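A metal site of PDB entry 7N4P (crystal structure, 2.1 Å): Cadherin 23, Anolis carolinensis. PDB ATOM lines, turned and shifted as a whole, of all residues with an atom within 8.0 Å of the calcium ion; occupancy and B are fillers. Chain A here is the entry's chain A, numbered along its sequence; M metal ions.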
ATOM      1  N   MET A   1     -27.782  10.984  10.432  1.00  0.00           N
ATOM      2  CA  MET A   1     -28.259  10.211  11.602  1.00  0.00           C
ATOM      3  C   MET A   1     -27.224   9.104  11.922  1.00  0.00           C
ATOM      4  O   MET A   1     -26.486   8.653  10.995  1.00  0.00           O
ATOM      5  CB  MET A   1     -29.639   9.595  11.347  1.00  0.00           C
ATOM      6  CG  MET A   1     -29.803   8.965   9.950  1.00  0.00           C
ATOM      7  SD  MET A   1     -31.416   8.172   9.668  1.00  0.00           S
ATOM      8  CE  MET A   1     -31.394   7.964   7.890  1.00  0.00           C
ATOM      9  N   ASN A   2     -27.175   8.699  13.186  1.00  0.00           N
ATOM     10  CA  ASN A   2     -26.412   7.503  13.646  1.00  0.00           C
ATOM     11  C   ASN A   2     -27.071   6.237  13.109  1.00  0.00           C
ATOM     12  O   ASN A   2     -28.305   6.225  12.970  1.00  0.00           O
ATOM     13  CB  ASN A   2     -26.399   7.398  15.162  1.00  0.00           C
ATOM     14  CG  ASN A   2     -25.728   6.122  15.600  1.00  0.00           C
ATOM     15  OD1 ASN A   2     -24.646   5.830  15.101  1.00  0.00           O
ATOM     16  ND2 ASN A   2     -26.369   5.347  16.456  1.00  0.00           N
ATOM     17  N   ARG A   3     -26.282   5.193  12.836  1.00  0.00           N
ATOM     18  CA  ARG A   3     -26.798   3.839  12.549  1.00  0.00           C
ATOM     19  C   ARG A   3     -26.478   2.904  13.720  1.00  0.00           C
ATOM     20  O   ARG A   3     -25.298   2.902  14.169  1.00  0.00           O
ATOM     21  CB  ARG A   3     -26.223   3.342  11.226  1.00  0.00           C
ATOM     22  CG  ARG A   3     -27.163   3.617  10.063  1.00  0.00           C
ATOM     23  CD  ARG A   3     -27.586   5.081  10.084  1.00  0.00           C
ATOM     24  NE  ARG A   3     -26.474   5.904   9.634  1.00  0.00           N
ATOM     25  CZ  ARG A   3     -26.288   6.256   8.351  1.00  0.00           C
ATOM     26  NH1 ARG A   3     -25.240   6.986   8.043  1.00  0.00           N
ATOM     27  NH2 ARG A   3     -27.168   5.883   7.403  1.00  0.00           N
ATOM     28  N   LEU A   4     -27.495   2.179  14.185  1.00  0.00           N
ATOM     29  CA  LEU A   4     -27.380   1.143  15.260  1.00  0.00           C
ATOM     30  C   LEU A   4     -26.474   0.039  14.764  1.00  0.00           C
ATOM     31  O   LEU A   4     -26.387  -0.191  13.570  1.00  0.00           O
ATOM     32  CB  LEU A   4     -28.761   0.666  15.705  1.00  0.00           C
ATOM     33  CG  LEU A   4     -29.586   1.797  16.300  1.00  0.00           C
ATOM     34  CD1 LEU A   4     -30.980   1.361  16.679  1.00  0.00           C
ATOM     35  CD2 LEU A   4     -28.822   2.394  17.494  1.00  0.00           C
ATOM     36  N   PRO A   5     -25.656  -0.539  15.673  1.00  0.00           N
ATOM     37  CA  PRO A   5     -24.773  -1.653  15.302  1.00  0.00           C
ATOM     38  C   PRO A   5     -25.666  -2.902  15.227  1.00  0.00           C
ATOM     39  O   PRO A   5     -26.773  -2.900  15.758  1.00  0.00           O
ATOM     40  CB  PRO A   5     -23.834  -1.768  16.503  1.00  0.00           C
ATOM     41  CG  PRO A   5     -24.750  -1.352  17.690  1.00  0.00           C
ATOM     42  CD  PRO A   5     -25.653  -0.273  17.125  1.00  0.00           C
ATOM     43  N   TYR A   6     -25.062  -3.957  14.713  1.00  0.00           N
ATOM     44  CA  TYR A   6     -25.673  -5.261  14.423  1.00  0.00           C
ATOM     45  C   TYR A   6     -24.637  -6.324  14.771  1.00  0.00           C
ATOM     46  O   TYR A   6     -23.408  -6.141  14.500  1.00  0.00           O
ATOM     47  CB  TYR A   6     -26.186  -5.318  12.975  1.00  0.00           C
ATOM     48  CG  TYR A   6     -25.130  -4.974  11.960  1.00  0.00           C
ATOM     49  CD1 TYR A   6     -24.814  -3.654  11.656  1.00  0.00           C
ATOM     50  CD2 TYR A   6     -24.416  -5.963  11.313  1.00  0.00           C
ATOM     51  CE1 TYR A   6     -23.834  -3.347  10.727  1.00  0.00           C
ATOM     52  CE2 TYR A   6     -23.425  -5.676  10.393  1.00  0.00           C
ATOM     53  CZ  TYR A   6     -23.140  -4.356  10.101  1.00  0.00           C
ATOM     54  OH  TYR A   6     -22.153  -4.087   9.189  1.00  0.00           O
ATOM     55  N   ARG A  34     -20.678  -4.830  14.264  1.00  0.00           N
ATOM     56  CA  ARG A  34     -20.195  -3.827  13.304  1.00  0.00           C
ATOM     57  C   ARG A  34     -21.151  -2.668  13.405  1.00  0.00           C
ATOM     58  O   ARG A  34     -22.246  -2.811  14.016  1.00  0.00           O
ATOM     59  CB  ARG A  34     -20.230  -4.281  11.860  1.00  0.00           C
ATOM     60  CG  ARG A  34     -19.200  -5.325  11.484  1.00  0.00           C
ATOM     61  CD  ARG A  34     -17.824  -4.856  11.834  1.00  0.00           C
ATOM     62  NE  ARG A  34     -16.747  -5.800  11.590  1.00  0.00           N
ATOM     63  CZ  ARG A  34     -16.232  -6.649  12.475  1.00  0.00           C
ATOM     64  NH1 ARG A  34     -16.703  -6.737  13.710  1.00  0.00           N
ATOM     65  NH2 ARG A  34     -15.230  -7.433  12.105  1.00  0.00           N
ATOM     66  N   ASP A  35     -20.680  -1.550  12.898  1.00  0.00           N
ATOM     67  CA  ASP A  35     -21.398  -0.272  12.998  1.00  0.00           C
ATOM     68  C   ASP A  35     -20.877   0.649  11.884  1.00  0.00           C
ATOM     69  O   ASP A  35     -19.648   0.836  11.704  1.00  0.00           O
ATOM     70  CB  ASP A  35     -21.295   0.199  14.434  1.00  0.00           C
ATOM     71  CG  ASP A  35     -21.934   1.538  14.664  1.00  0.00           C
ATOM     72  OD1 ASP A  35     -21.514   2.482  13.955  1.00  0.00           O
ATOM     73  OD2 ASP A  35     -22.782   1.629  15.605  1.00  0.00           O
ATOM     74  N   LEU A  36     -21.827   1.230  11.160  1.00  0.00           N
ATOM     75  CA  LEU A  36     -21.563   2.056   9.965  1.00  0.00           C
ATOM     76  C   LEU A  36     -20.649   3.240  10.343  1.00  0.00           C
ATOM     77  O   LEU A  36     -19.652   3.444   9.624  1.00  0.00           O
ATOM     78  CB  LEU A  36     -22.924   2.476   9.381  1.00  0.00           C
ATOM     79  CG  LEU A  36     -22.854   3.136   8.019  1.00  0.00           C
ATOM     80  CD1 LEU A  36     -21.738   2.516   7.171  1.00  0.00           C
ATOM     81  CD2 LEU A  36     -24.201   3.005   7.306  1.00  0.00           C
ATOM     82  N   ASP A  37     -20.960   3.982  11.425  1.00  0.00           N
ATOM     83  CA  ASP A  37     -20.159   5.107  12.003  1.00  0.00           C
ATOM     84  C   ASP A  37     -18.779   4.648  12.529  1.00  0.00           C
ATOM     85  O   ASP A  37     -18.016   5.468  13.073  1.00  0.00           O
ATOM     86  CB  ASP A  37     -20.967   5.793  13.122  1.00  0.00           C
ATOM     87  CG  ASP A  37     -22.467   5.739  12.815  1.00  0.00           C
ATOM     88  OD1 ASP A  37     -23.107   4.786  13.246  1.00  0.00           O
ATOM     89  OD2 ASP A  37     -22.954   6.630  12.094  1.00  0.00           O
ATOM     90  N   ASN A  38     -18.437   3.360  12.420  1.00  0.00           N
ATOM     91  CA  ASN A  38     -17.277   2.783  13.143  1.00  0.00           C
ATOM     92  C   ASN A  38     -17.253   3.227  14.637  1.00  0.00           C
ATOM     93  O   ASN A  38     -16.138   3.444  15.161  1.00  0.00           O
ATOM     94  CB  ASN A  38     -16.011   3.137  12.351  1.00  0.00           C
ATOM     95  CG  ASN A  38     -14.850   2.227  12.700  1.00  0.00           C
ATOM     96  OD1 ASN A  38     -13.781   2.694  13.116  1.00  0.00           O
ATOM     97  ND2 ASN A  38     -15.075   0.928  12.569  1.00  0.00           N
ATOM     98  N   ASP A  39     -18.394   3.359  15.332  1.00  0.00           N
ATOM     99  CA  ASP A  39     -18.410   3.743  16.769  1.00  0.00           C
ATOM    100  C   ASP A  39     -17.835   2.622  17.663  1.00  0.00           C
ATOM    101  O   ASP A  39     -17.999   1.432  17.375  1.00  0.00           O
ATOM    102  CB  ASP A  39     -19.823   4.004  17.282  1.00  0.00           C
ATOM    103  CG  ASP A  39     -20.572   5.039  16.498  1.00  0.00           C
ATOM    104  OD1 ASP A  39     -19.916   5.990  16.016  1.00  0.00           O
ATOM    105  OD2 ASP A  39     -21.783   4.873  16.368  1.00  0.00           O
ATOM    106  N   PRO A  40     -17.160   2.994  18.806  1.00  0.00           N
ATOM    107  CA  PRO A  40     -16.760   2.021  19.817  1.00  0.00           C
ATOM    108  C   PRO A  40     -18.039   1.372  20.396  1.00  0.00           C
ATOM    109  O   PRO A  40     -19.043   2.131  20.629  1.00  0.00           O
ATOM    110  CB  PRO A  40     -15.913   2.811  20.827  1.00  0.00           C
ATOM    111  CG  PRO A  40     -15.640   4.147  20.146  1.00  0.00           C
ATOM    112  CD  PRO A  40     -16.797   4.366  19.200  1.00  0.00           C
ATOM    113  N   LEU A  41     -18.049   0.029  20.497  1.00  0.00           N
ATOM    114  CA  LEU A  41     -19.224  -0.754  20.961  1.00  0.00           C
ATOM    115  C   LEU A  41     -19.025  -1.305  22.392  1.00  0.00           C
ATOM    116  O   LEU A  41     -17.881  -1.726  22.718  1.00  0.00           O
ATOM    117  CB  LEU A  41     -19.517  -1.892  19.974  1.00  0.00           C
ATOM    118  CG  LEU A  41     -19.790  -1.415  18.544  1.00  0.00           C
ATOM    119  CD1 LEU A  41     -20.303  -2.563  17.700  1.00  0.00           C
ATOM    120  CD2 LEU A  41     -20.784  -0.288  18.554  1.00  0.00           C
ATOM    121  N   SER A  84     -24.337  -2.134  21.796  1.00  0.00           N
ATOM    122  CA  SER A  84     -24.682  -0.702  21.856  1.00  0.00           C
ATOM    123  C   SER A  84     -23.533   0.148  21.328  1.00  0.00           C
ATOM    124  O   SER A  84     -22.340  -0.182  21.604  1.00  0.00           O
ATOM    125  CB  SER A  84     -25.068  -0.350  23.233  1.00  0.00           C
ATOM    126  OG  SER A  84     -25.615   0.926  23.222  1.00  0.00           O
ATOM    127  N   ASP A  85     -23.905   1.197  20.590  1.00  0.00           N
ATOM    128  CA  ASP A  85     -23.126   2.436  20.353  1.00  0.00           C
ATOM    129  C   ASP A  85     -23.567   3.438  21.446  1.00  0.00           C
ATOM    130  O   ASP A  85     -24.446   3.078  22.294  1.00  0.00           O
ATOM    131  CB  ASP A  85     -23.344   2.916  18.904  1.00  0.00           C
ATOM    132  CG  ASP A  85     -24.767   3.277  18.518  1.00  0.00           C
ATOM    133  OD1 ASP A  85     -25.620   3.361  19.438  1.00  0.00           O
ATOM    134  OD2 ASP A  85     -25.023   3.518  17.294  1.00  0.00           O
ATOM    135  N   SER A  86     -23.085   4.675  21.385  1.00  0.00           N
ATOM    136  CA  SER A  86     -23.613   5.773  22.246  1.00  0.00           C
ATOM    137  C   SER A  86     -25.153   5.644  22.427  1.00  0.00           C
ATOM    138  O   SER A  86     -25.614   5.531  23.580  1.00  0.00           O
ATOM    139  CB  SER A  86     -23.187   7.130  21.660  1.00  0.00           C
ATOM    140  OG  SER A  86     -23.808   8.248  22.315  1.00  0.00           O
ATOM    141  N   GLN A  87     -25.915   5.516  21.330  1.00  0.00           N
ATOM    142  CA  GLN A  87     -27.287   6.085  21.176  1.00  0.00           C
ATOM    143  C   GLN A  87     -28.409   5.049  21.322  1.00  0.00           C
ATOM    144  O   GLN A  87     -29.567   5.462  21.627  1.00  0.00           O
ATOM    145  CB  GLN A  87     -27.298   6.710  19.796  1.00  0.00           C
ATOM    146  CG  GLN A  87     -25.989   7.449  19.577  1.00  0.00           C
ATOM    147  CD  GLN A  87     -26.156   8.609  18.643  1.00  0.00           C
ATOM    148  OE1 GLN A  87     -25.423   8.740  17.684  1.00  0.00           O
ATOM    149  NE2 GLN A  87     -27.145   9.441  18.923  1.00  0.00           N
ATOM    150  N   GLY A  88     -28.118   3.782  21.106  1.00  0.00           N
ATOM    151  CA  GLY A  88     -29.123   2.745  21.329  1.00  0.00           C
ATOM    152  C   GLY A  88     -28.504   1.385  21.541  1.00  0.00           C
ATOM    153  O   GLY A  88     -27.259   1.233  21.240  1.00  0.00           O
HETATM  154 CA    CA M   1     -23.408   3.720  15.350  1.00  0.00          CA
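NE of Arg 3 lies within hydrogen-bond range of O of Met 1 (3.1 Å). The side-chain carboxylate of Asp 85 is in hydrogen-bond range of the backbone NH of Gln 87 (2.9 Å). The side-chain carboxylate of Asp 85 sits at hydrogen-bond distance from the backbone NH of Gly 88 (3.0 Å).
The calcium ion is bound by OD2 of Asp 35 (2.2 Å), OD2 of Asp 39 (2.2 Å), O of Arg 3 (2.4 Å), OD1 of Asp 37 (2.4 Å), OD1 of Asn 2 (2.5 Å), OD2 of Asp 85 (2.5 Å) and OD1 of Asp 35 (2.7 Å). The calcium ion has seven donor atoms within binding distance.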
